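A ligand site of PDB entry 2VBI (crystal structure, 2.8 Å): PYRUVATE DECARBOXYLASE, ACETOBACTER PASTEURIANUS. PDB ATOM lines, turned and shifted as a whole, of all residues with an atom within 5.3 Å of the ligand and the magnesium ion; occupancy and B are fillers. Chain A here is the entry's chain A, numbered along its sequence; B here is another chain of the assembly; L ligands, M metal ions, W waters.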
ATOM      1  N   GLU A 383      33.044   9.122  -2.078  1.00  0.00           N
ATOM      2  CA  GLU A 383      31.862   9.964  -2.199  1.00  0.00           C
ATOM      3  C   GLU A 383      30.575   9.266  -1.764  1.00  0.00           C
ATOM      4  O   GLU A 383      30.480   8.031  -1.798  1.00  0.00           O
ATOM      5  CB  GLU A 383      31.733  10.458  -3.649  1.00  0.00           C
ATOM      6  CG  GLU A 383      30.568  11.387  -3.909  1.00  0.00           C
ATOM      7  CD  GLU A 383      30.667  12.680  -3.146  1.00  0.00           C
ATOM      8  OE1 GLU A 383      30.303  12.703  -1.952  1.00  0.00           O
ATOM      9  OE2 GLU A 383      31.117  13.682  -3.757  1.00  0.00           O
ATOM     10  N   THR A 384      29.586  10.072  -1.371  1.00  0.00           N
ATOM     11  CA  THR A 384      28.229   9.601  -1.138  1.00  0.00           C
ATOM     12  C   THR A 384      27.687   8.945  -2.415  1.00  0.00           C
ATOM     13  O   THR A 384      27.831   9.475  -3.513  1.00  0.00           O
ATOM     14  CB  THR A 384      27.316  10.745  -0.690  1.00  0.00           C
ATOM     15  OG1 THR A 384      27.883  11.379   0.465  1.00  0.00           O
ATOM     16  CG2 THR A 384      25.915  10.235  -0.339  1.00  0.00           C
ATOM     17  N   GLY A 385      27.071   7.782  -2.245  1.00  0.00           N
ATOM     18  CA  GLY A 385      26.628   6.943  -3.364  1.00  0.00           C
ATOM     19  C   GLY A 385      27.164   5.553  -3.132  1.00  0.00           C
ATOM     20  O   GLY A 385      27.570   5.217  -2.013  1.00  0.00           O
ATOM     21  N   ASP A 386      27.203   4.736  -4.178  1.00  0.00           N
ATOM     22  CA  ASP A 386      27.690   3.363  -4.037  1.00  0.00           C
ATOM     23  C   ASP A 386      29.166   3.307  -3.628  1.00  0.00           C
ATOM     24  O   ASP A 386      29.640   2.268  -3.159  1.00  0.00           O
ATOM     25  CB  ASP A 386      27.437   2.547  -5.326  1.00  0.00           C
ATOM     26  CG  ASP A 386      27.476   1.039  -5.087  1.00  0.00           C
ATOM     27  OD1 ASP A 386      27.157   0.597  -3.958  1.00  0.00           O
ATOM     28  OD2 ASP A 386      27.817   0.281  -6.039  1.00  0.00           O
ATOM     29  N   SER A 387      29.879   4.414  -3.778  1.00  0.00           N
ATOM     30  CA  SER A 387      31.274   4.476  -3.363  1.00  0.00           C
ATOM     31  C   SER A 387      31.444   4.312  -1.847  1.00  0.00           C
ATOM     32  O   SER A 387      32.469   3.811  -1.403  1.00  0.00           O
ATOM     33  CB  SER A 387      31.944   5.759  -3.846  1.00  0.00           C
ATOM     34  OG  SER A 387      31.886   5.836  -5.253  1.00  0.00           O
ATOM     35  N   GLY A 409      26.836  14.280   4.037  1.00  0.00           N
ATOM     36  CA  GLY A 409      26.430  13.567   2.810  1.00  0.00           C
ATOM     37  C   GLY A 409      26.043  14.432   1.619  1.00  0.00           C
ATOM     38  O   GLY A 409      25.048  14.161   0.948  1.00  0.00           O
ATOM     39  N   HIS A 410      26.830  15.480   1.377  1.00  0.00           N
ATOM     40  CA  HIS A 410      26.618  16.396   0.274  1.00  0.00           C
ATOM     41  C   HIS A 410      27.339  15.844  -0.948  1.00  0.00           C
ATOM     42  O   HIS A 410      28.581  15.914  -1.007  1.00  0.00           O
ATOM     43  CB  HIS A 410      27.206  17.767   0.632  1.00  0.00           C
ATOM     44  CG  HIS A 410      26.937  18.834  -0.372  1.00  0.00           C
ATOM     45  ND1 HIS A 410      27.467  18.815  -1.651  1.00  0.00           N
ATOM     46  CD2 HIS A 410      26.203  19.975  -0.292  1.00  0.00           C
ATOM     47  CE1 HIS A 410      27.062  19.884  -2.313  1.00  0.00           C
ATOM     48  NE2 HIS A 410      26.306  20.612  -1.511  1.00  0.00           N
ATOM     49  N   ILE A 411      26.606  15.307  -1.916  1.00  0.00           N
ATOM     50  CA  ILE A 411      27.248  14.808  -3.134  1.00  0.00           C
ATOM     51  C   ILE A 411      28.059  15.906  -3.820  1.00  0.00           C
ATOM     52  O   ILE A 411      27.685  17.072  -3.810  1.00  0.00           O
ATOM     53  CB  ILE A 411      26.235  14.168  -4.131  1.00  0.00           C
ATOM     54  CG1 ILE A 411      25.238  15.195  -4.646  1.00  0.00           C
ATOM     55  CG2 ILE A 411      25.533  12.963  -3.495  1.00  0.00           C
ATOM     56  CD1 ILE A 411      24.428  14.722  -5.823  1.00  0.00           C
ATOM     57  N   VAL A 434      34.379   8.596  -6.967  1.00  0.00           N
ATOM     58  CA  VAL A 434      33.270   9.528  -7.138  1.00  0.00           C
ATOM     59  C   VAL A 434      32.319   9.068  -8.230  1.00  0.00           C
ATOM     60  O   VAL A 434      32.750   8.645  -9.288  1.00  0.00           O
ATOM     61  CB  VAL A 434      33.761  10.987  -7.375  1.00  0.00           C
ATOM     62  CG1 VAL A 434      34.554  11.112  -8.655  1.00  0.00           C
ATOM     63  CG2 VAL A 434      32.599  11.972  -7.374  1.00  0.00           C
ATOM     64  N   GLY A 435      31.020   9.154  -7.950  1.00  0.00           N
ATOM     65  CA  GLY A 435      30.004   8.787  -8.934  1.00  0.00           C
ATOM     66  C   GLY A 435      29.825   9.873  -9.956  1.00  0.00           C
ATOM     67  O   GLY A 435      30.244  11.011  -9.762  1.00  0.00           O
ATOM     68  N   ASP A 436      29.190   9.510 -11.078  1.00  0.00           N
ATOM     69  CA  ASP A 436      28.995  10.450 -12.169  1.00  0.00           C
ATOM     70  C   ASP A 436      28.065  11.595 -11.768  1.00  0.00           C
ATOM     71  O   ASP A 436      28.297  12.744 -12.140  1.00  0.00           O
ATOM     72  CB  ASP A 436      28.522   9.744 -13.451  1.00  0.00           C
ATOM     73  CG  ASP A 436      27.227   8.941 -13.263  1.00  0.00           C
ATOM     74  OD1 ASP A 436      26.972   8.426 -12.159  1.00  0.00           O
ATOM     75  OD2 ASP A 436      26.483   8.818 -14.252  1.00  0.00           O
ATOM     76  N   GLY A 437      27.039  11.274 -10.987  1.00  0.00           N
ATOM     77  CA  GLY A 437      26.082  12.272 -10.538  1.00  0.00           C
ATOM     78  C   GLY A 437      26.714  13.295  -9.627  1.00  0.00           C
ATOM     79  O   GLY A 437      26.466  14.493  -9.742  1.00  0.00           O
ATOM     80  N   SER A 438      27.539  12.797  -8.700  1.00  0.00           N
ATOM     81  CA  SER A 438      28.215  13.665  -7.741  1.00  0.00           C
ATOM     82  C   SER A 438      29.220  14.573  -8.415  1.00  0.00           C
ATOM     83  O   SER A 438      29.340  15.744  -8.063  1.00  0.00           O
ATOM     84  CB  SER A 438      28.924  12.824  -6.672  1.00  0.00           C
ATOM     85  OG  SER A 438      27.996  12.002  -5.982  1.00  0.00           O
ATOM     86  N   PHE A 439      29.936  14.013  -9.380  1.00  0.00           N
ATOM     87  CA  PHE A 439      30.990  14.738 -10.048  1.00  0.00           C
ATOM     88  C   PHE A 439      30.465  16.009 -10.691  1.00  0.00           C
ATOM     89  O   PHE A 439      31.149  17.033 -10.682  1.00  0.00           O
ATOM     90  CB  PHE A 439      31.675  13.845 -11.078  1.00  0.00           C
ATOM     91  CG  PHE A 439      32.904  14.441 -11.682  1.00  0.00           C
ATOM     92  CD1 PHE A 439      34.108  14.437 -10.994  1.00  0.00           C
ATOM     93  CD2 PHE A 439      32.865  15.010 -12.944  1.00  0.00           C
ATOM     94  CE1 PHE A 439      35.258  14.989 -11.555  1.00  0.00           C
ATOM     95  CE2 PHE A 439      34.007  15.569 -13.515  1.00  0.00           C
ATOM     96  CZ  PHE A 439      35.209  15.562 -12.818  1.00  0.00           C
ATOM     97  N   LEU A 441      28.274  18.165  -9.789  1.00  0.00           N
ATOM     98  CA  LEU A 441      28.075  19.311  -8.892  1.00  0.00           C
ATOM     99  C   LEU A 441      29.298  20.191  -8.718  1.00  0.00           C
ATOM    100  O   LEU A 441      29.177  21.402  -8.574  1.00  0.00           O
ATOM    101  CB  LEU A 441      27.614  18.856  -7.515  1.00  0.00           C
ATOM    102  CG  LEU A 441      26.130  18.531  -7.361  1.00  0.00           C
ATOM    103  CD1 LEU A 441      25.833  17.099  -7.781  1.00  0.00           C
ATOM    104  CD2 LEU A 441      25.703  18.763  -5.938  1.00  0.00           C
ATOM    105  N   ILE A 461      33.088   6.807 -11.349  1.00  0.00           N
ATOM    106  CA  ILE A 461      32.217   5.649 -11.587  1.00  0.00           C
ATOM    107  C   ILE A 461      31.007   6.075 -12.423  1.00  0.00           C
ATOM    108  O   ILE A 461      30.003   6.559 -11.893  1.00  0.00           O
ATOM    109  CB  ILE A 461      31.752   4.953 -10.268  1.00  0.00           C
ATOM    110  CG1 ILE A 461      32.884   4.885  -9.228  1.00  0.00           C
ATOM    111  CG2 ILE A 461      31.157   3.574 -10.576  1.00  0.00           C
ATOM    112  CD1 ILE A 461      34.096   4.025  -9.606  1.00  0.00           C
ATOM    113  N   ASN A 463      28.016   5.118 -14.038  1.00  0.00           N
ATOM    114  CA  ASN A 463      26.945   4.128 -14.178  1.00  0.00           C
ATOM    115  C   ASN A 463      25.646   4.736 -14.704  1.00  0.00           C
ATOM    116  O   ASN A 463      24.593   4.112 -14.639  1.00  0.00           O
ATOM    117  CB  ASN A 463      26.729   3.344 -12.885  1.00  0.00           C
ATOM    118  CG  ASN A 463      26.509   4.238 -11.673  1.00  0.00           C
ATOM    119  OD1 ASN A 463      26.172   5.416 -11.792  1.00  0.00           O
ATOM    120  ND2 ASN A 463      26.682   3.668 -10.493  1.00  0.00           N
ATOM    121  N   ARG A 464      25.737   5.969 -15.215  1.00  0.00           N
ATOM    122  CA  ARG A 464      24.643   6.657 -15.897  1.00  0.00           C
ATOM    123  C   ARG A 464      23.471   7.068 -15.015  1.00  0.00           C
ATOM    124  O   ARG A 464      22.307   6.913 -15.406  1.00  0.00           O
ATOM    125  CB  ARG A 464      24.123   5.822 -17.085  1.00  0.00           C
ATOM    126  CG  ARG A 464      25.142   5.511 -18.134  1.00  0.00           C
ATOM    127  CD  ARG A 464      25.564   6.760 -18.887  1.00  0.00           C
ATOM    128  NE  ARG A 464      26.304   6.383 -20.083  1.00  0.00           N
ATOM    129  CZ  ARG A 464      25.804   6.402 -21.318  1.00  0.00           C
ATOM    130  NH1 ARG A 464      24.559   6.801 -21.519  1.00  0.00           N
ATOM    131  NH2 ARG A 464      26.563   6.036 -22.343  1.00  0.00           N
ATOM    132  N   GLY A 465      23.775   7.603 -13.831  1.00  0.00           N
ATOM    133  CA  GLY A 465      22.740   8.154 -12.966  1.00  0.00           C
ATOM    134  C   GLY A 465      22.949   7.971 -11.483  1.00  0.00           C
ATOM    135  O   GLY A 465      23.985   7.476 -11.033  1.00  0.00           O
ATOM    136  N   TYR A 466      21.930   8.400 -10.736  1.00  0.00           N
ATOM    137  CA  TYR A 466      21.906   8.305  -9.289  1.00  0.00           C
ATOM    138  C   TYR A 466      21.478   6.890  -8.903  1.00  0.00           C
ATOM    139  O   TYR A 466      20.326   6.650  -8.552  1.00  0.00           O
ATOM    140  CB  TYR A 466      20.915   9.306  -8.693  1.00  0.00           C
ATOM    141  CG  TYR A 466      21.137  10.784  -9.021  1.00  0.00           C
ATOM    142  CD1 TYR A 466      22.412  11.277  -9.307  1.00  0.00           C
ATOM    143  CD2 TYR A 466      20.062  11.679  -8.992  1.00  0.00           C
ATOM    144  CE1 TYR A 466      22.613  12.635  -9.575  1.00  0.00           C
ATOM    145  CE2 TYR A 466      20.254  13.040  -9.261  1.00  0.00           C
ATOM    146  CZ  TYR A 466      21.528  13.499  -9.549  1.00  0.00           C
ATOM    147  OH  TYR A 466      21.733  14.833  -9.814  1.00  0.00           O
ATOM    148  N   VAL A 467      22.420   5.952  -8.985  1.00  0.00           N
ATOM    149  CA  VAL A 467      22.110   4.523  -8.798  1.00  0.00           C
ATOM    150  C   VAL A 467      21.660   4.190  -7.373  1.00  0.00           C
ATOM    151  O   VAL A 467      20.718   3.410  -7.192  1.00  0.00           O
ATOM    152  CB  VAL A 467      23.266   3.621  -9.280  1.00  0.00           C
ATOM    153  CG1 VAL A 467      23.116   2.196  -8.755  1.00  0.00           C
ATOM    154  CG2 VAL A 467      23.307   3.613 -10.785  1.00  0.00           C
ATOM    155  N   ILE A 468      22.318   4.800  -6.372  1.00  0.00           N
ATOM    156  CA  ILE A 468      21.923   4.641  -4.969  1.00  0.00           C
ATOM    157  C   ILE A 468      20.438   4.951  -4.785  1.00  0.00           C
ATOM    158  O   ILE A 468      19.809   4.469  -3.843  1.00  0.00           O
ATOM    159  CB  ILE A 468      22.771   5.522  -4.013  1.00  0.00           C
ATOM    160  CG1 ILE A 468      22.448   5.205  -2.545  1.00  0.00           C
ATOM    161  CG2 ILE A 468      22.561   6.998  -4.331  1.00  0.00           C
ATOM    162  CD1 ILE A 468      23.476   5.720  -1.548  1.00  0.00           C
ATOM    163  N   GLU A 469      19.895   5.729  -5.702  1.00  0.00           N
ATOM    164  CA  GLU A 469      18.510   6.164  -5.637  1.00  0.00           C
ATOM    165  C   GLU A 469      17.638   5.323  -6.539  1.00  0.00           C
ATOM    166  O   GLU A 469      16.503   4.999  -6.184  1.00  0.00           O
ATOM    167  CB  GLU A 469      18.419   7.632  -6.010  1.00  0.00           C
ATOM    168  CG  GLU A 469      17.516   8.428  -5.093  1.00  0.00           C
ATOM    169  CD  GLU A 469      18.056   8.534  -3.651  1.00  0.00           C
ATOM    170  OE1 GLU A 469      17.534   7.794  -2.773  1.00  0.00           O
ATOM    171  OE2 GLU A 469      18.987   9.367  -3.424  1.00  0.00           O
ATOM    172  N   VAL B  24      16.324  19.118  -7.762  1.00  0.00           N
ATOM    173  CA  VAL B  24      17.394  18.153  -7.622  1.00  0.00           C
ATOM    174  C   VAL B  24      16.927  17.110  -6.617  1.00  0.00           C
ATOM    175  O   VAL B  24      16.501  17.460  -5.498  1.00  0.00           O
ATOM    176  CB  VAL B  24      18.703  18.787  -7.131  1.00  0.00           C
ATOM    177  CG1 VAL B  24      19.793  17.744  -7.005  1.00  0.00           C
ATOM    178  CG2 VAL B  24      19.141  19.890  -8.076  1.00  0.00           C
ATOM    179  N   ALA B  25      16.991  15.841  -7.011  1.00  0.00           N
ATOM    180  CA  ALA B  25      16.471  14.739  -6.202  1.00  0.00           C
ATOM    181  C   ALA B  25      17.289  14.493  -4.944  1.00  0.00           C
ATOM    182  O   ALA B  25      18.503  14.665  -4.938  1.00  0.00           O
ATOM    183  CB  ALA B  25      16.396  13.472  -7.015  1.00  0.00           C
ATOM    184  N   GLY B  26      16.612  14.101  -3.869  1.00  0.00           N
ATOM    185  CA  GLY B  26      17.242  13.633  -2.656  1.00  0.00           C
ATOM    186  C   GLY B  26      16.223  12.844  -1.885  1.00  0.00           C
ATOM    187  O   GLY B  26      15.014  13.062  -2.049  1.00  0.00           O
ATOM    188  N   ASP B  27      16.671  11.946  -1.021  1.00  0.00           N
ATOM    189  CA  ASP B  27      15.730  11.043  -0.343  1.00  0.00           C
ATOM    190  C   ASP B  27      14.608  11.764   0.437  1.00  0.00           C
ATOM    191  O   ASP B  27      13.469  11.269   0.489  1.00  0.00           O
ATOM    192  CB  ASP B  27      16.450   9.955   0.484  1.00  0.00           C
ATOM    193  CG  ASP B  27      17.269  10.522   1.644  1.00  0.00           C
ATOM    194  OD1 ASP B  27      17.621  11.727   1.642  1.00  0.00           O
ATOM    195  OD2 ASP B  27      17.579   9.736   2.565  1.00  0.00           O
ATOM    196  N   GLU B  50      22.223  22.545  -6.593  1.00  0.00           N
ATOM    197  CA  GLU B  50      21.161  23.336  -6.014  1.00  0.00           C
ATOM    198  C   GLU B  50      21.351  24.839  -6.144  1.00  0.00           C
ATOM    199  O   GLU B  50      20.366  25.586  -6.217  1.00  0.00           O
ATOM    200  CB  GLU B  50      20.932  22.943  -4.556  1.00  0.00           C
ATOM    201  CG  GLU B  50      20.341  21.546  -4.403  1.00  0.00           C
ATOM    202  CD  GLU B  50      21.368  20.423  -4.418  1.00  0.00           C
ATOM    203  OE1 GLU B  50      22.589  20.707  -4.575  1.00  0.00           O
ATOM    204  OE2 GLU B  50      20.952  19.259  -4.262  1.00  0.00           O
ATOM    205  N   THR B  72      16.582  19.068  -1.548  1.00  0.00           N
ATOM    206  CA  THR B  72      16.623  18.238  -0.360  1.00  0.00           C
ATOM    207  C   THR B  72      17.170  19.028   0.837  1.00  0.00           C
ATOM    208  O   THR B  72      17.821  20.062   0.659  1.00  0.00           O
ATOM    209  CB  THR B  72      17.427  16.933  -0.597  1.00  0.00           C
ATOM    210  OG1 THR B  72      17.158  16.012   0.472  1.00  0.00           O
ATOM    211  CG2 THR B  72      18.912  17.206  -0.705  1.00  0.00           C
ATOM    212  N   VAL B  75      21.788  20.040   2.715  1.00  0.00           N
ATOM    213  CA  VAL B  75      22.823  19.927   1.688  1.00  0.00           C
ATOM    214  C   VAL B  75      22.369  20.563   0.367  1.00  0.00           C
ATOM    215  O   VAL B  75      23.184  21.140  -0.361  1.00  0.00           O
ATOM    216  CB  VAL B  75      23.315  18.472   1.496  1.00  0.00           C
ATOM    217  CG1 VAL B  75      24.040  18.019   2.745  1.00  0.00           C
ATOM    218  CG2 VAL B  75      22.181  17.524   1.163  1.00  0.00           C
ATOM    219  N   GLY B  76      21.079  20.479   0.096  1.00  0.00           N
ATOM    220  CA  GLY B  76      20.498  21.168  -1.036  1.00  0.00           C
ATOM    221  C   GLY B  76      20.106  22.591  -0.673  1.00  0.00           C
ATOM    222  O   GLY B  76      20.557  23.561  -1.285  1.00  0.00           O
ATOM    223  N   HIS B 114      22.221  14.587   6.703  1.00  0.00           N
ATOM    224  CA  HIS B 114      22.079  15.935   6.144  1.00  0.00           C
ATOM    225  C   HIS B 114      21.788  16.999   7.209  1.00  0.00           C
ATOM    226  O   HIS B 114      21.267  18.070   6.905  1.00  0.00           O
ATOM    227  CB  HIS B 114      21.012  16.025   5.038  1.00  0.00           C
ATOM    228  CG  HIS B 114      21.252  15.114   3.879  1.00  0.00           C
ATOM    229  ND1 HIS B 114      22.489  14.599   3.568  1.00  0.00           N
ATOM    230  CD2 HIS B 114      20.405  14.655   2.928  1.00  0.00           C
ATOM    231  CE1 HIS B 114      22.388  13.831   2.491  1.00  0.00           C
ATOM    232  NE2 HIS B 114      21.132  13.853   2.081  1.00  0.00           N
HETATM  233  N1  LIG L   1      21.881  17.038  -3.369  1.00  0.00           N
HETATM  234  C1  LIG L   1      23.045  17.163  -2.620  1.00  0.00           C
HETATM  235  C2  LIG L   1      23.802  18.453  -2.648  1.00  0.00           C
HETATM  236  N2  LIG L   1      23.506  16.098  -1.869  1.00  0.00           N
HETATM  237  C3  LIG L   1      22.802  14.909  -1.847  1.00  0.00           C
HETATM  238  N3  LIG L   1      23.266  13.922  -1.099  1.00  0.00           N
HETATM  239  C4  LIG L   1      21.628  14.786  -2.598  1.00  0.00           C
HETATM  240  C5  LIG L   1      21.169  15.855  -3.357  1.00  0.00           C
HETATM  241  C6  LIG L   1      20.808  13.512  -2.619  1.00  0.00           C
HETATM  242  N4  LIG L   1      21.554  12.406  -3.184  1.00  0.00           N
HETATM  243  C7  LIG L   1      22.156  11.435  -2.402  1.00  0.00           C
HETATM  244  S1  LIG L   1      22.929  10.332  -3.254  1.00  0.00           S
HETATM  245  C8  LIG L   1      22.535  11.006  -4.647  1.00  0.00           C
HETATM  246  C9  LIG L   1      21.754  12.147  -4.511  1.00  0.00           C
HETATM  247  C10 LIG L   1      21.256  12.963  -5.676  1.00  0.00           C
HETATM  248  C11 LIG L   1      23.024  10.272  -5.875  1.00  0.00           C
HETATM  249  C12 LIG L   1      24.527  10.343  -6.152  1.00  0.00           C
HETATM  250  O1  LIG L   1      24.757   9.629  -7.348  1.00  0.00           O
HETATM  251  P1  LIG L   1      26.218   9.223  -7.921  1.00  0.00           P
HETATM  252  O2  LIG L   1      26.098   9.003  -9.406  1.00  0.00           O
HETATM  253  O3  LIG L   1      27.245  10.289  -7.641  1.00  0.00           O
HETATM  254  O4  LIG L   1      26.642   7.853  -7.194  1.00  0.00           O
HETATM  255  P2  LIG L   1      25.970   6.420  -7.537  1.00  0.00           P
HETATM  256  O5  LIG L   1      24.701   6.202  -6.746  1.00  0.00           O
HETATM  257  O6  LIG L   1      26.978   5.350  -7.167  1.00  0.00           O
HETATM  258  O7  LIG L   1      25.620   6.309  -9.007  1.00  0.00           O
HETATM  259 MG    MG M   1      26.256   7.498 -10.695  1.00  0.00          MG
HETATM  260  O   HOH W   1      28.093   6.163  -9.603  1.00  0.00           O
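Residues that only touch the ligand: Ala 25 of chain B (3.3 Å), Gly 435 (3.4 Å), Tyr 466 (3.5 Å), His 410 (3.5 Å), Gly 26 of chain B (3.6 Å), Val 75 of chain B (3.6 Å), His 114 of chain B (3.7 Å), Thr 72 of chain B (3.7 Å), Leu 441 (3.8 Å), Glu 469 (3.9 Å) and Gly 385 (3.9 Å).
Within 4 Å of the ligand: Gly 385, Asp 386, Gly 409, His 410, Ile 411, Gly 435, Asp 436, Gly 437, Ser 438, Leu 441, Asn 463, Gly 465, Tyr 466, Val 467, Ile 468, Glu 469, Ala 25 of chain B, Gly 26 of chain B, Glu 50 of chain B, Thr 72 of chain B, Val 75 of chain B and His 114 of chain B.
The nearest printed residue that does not touch the ligand is Thr 384 (4.2 Å).
The side-chain carboxylate (OD2) of Asp 436 is in hydrogen-bond range of the backbone NH (N) of Arg 464, at 3.1 Å.
A ring nitrogen (NE2) of His 410 sits close to the backbone carbonyl oxygen (O) of Val 75 of chain B (3.4 Å).
The backbone NH of Asp 436 is in hydrogen-bond range of the backbone carbonyl oxygen of Ile 461 (3.2 Å).
Water W1 lies within hydrogen-bond range of an oxygen (O6) of the ligand, the side-chain amide nitrogen of Asn 463 and the backbone carbonyl oxygen of Ile 461.
The side-chain carboxylate of Glu 50 of chain B sits at hydrogen-bond distance from a nitrogen (N1) of the ligand (2.6 Å).
N3 of the ligand sits at hydrogen-bond distance from O of Gly 409, at 2.7 Å.
N of Ser 438 lies within hydrogen-bond range of O3 of the ligand (2.7 Å).
The backbone NH (N) of Gly 437 sits at hydrogen-bond distance from an oxygen (O3) of the ligand, 3.5 Å away.
N of Ile 468 lies within hydrogen-bond range of O5 of the ligand (2.8 Å).
The backbone NH (N) of Val 467 is in hydrogen-bond range of an oxygen (O5) of the ligand, at 3.2 Å.
The backbone NH of Ile 411 lies within hydrogen-bond range of a nitrogen (N2) of the ligand, 3.2 Å away.
An oxygen (O6) of the ligand is in hydrogen-bond range of the backbone NH of Asp 386 (3.1 Å).
O3 of the ligand is in hydrogen-bond range of OG of Ser 438, 2.5 Å away.
Gly 437 touches the magnesium ion (N to MG, 3.9 Å).
Four residues have an atom within 4 Å of the magnesium ion: Asp 436, Gly 437, Asn 463 and Gly 465.
The nearest printed residue that does not touch the magnesium ion is Ile 461 (4.04 Å).
The magnesium ion is bound by OD1 of Asp 436 (1.9 Å).
O2 of the ligand is bound to the magnesium ion.
O7 of the ligand is bound to the magnesium ion.
The magnesium ion is bound by O of Gly 465, 2.3 Å away.
OD1 of Asn 463 is bound to the magnesium ion, 2.4 Å away.
The magnesium ion is bound by water W1 (2.5 Å).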
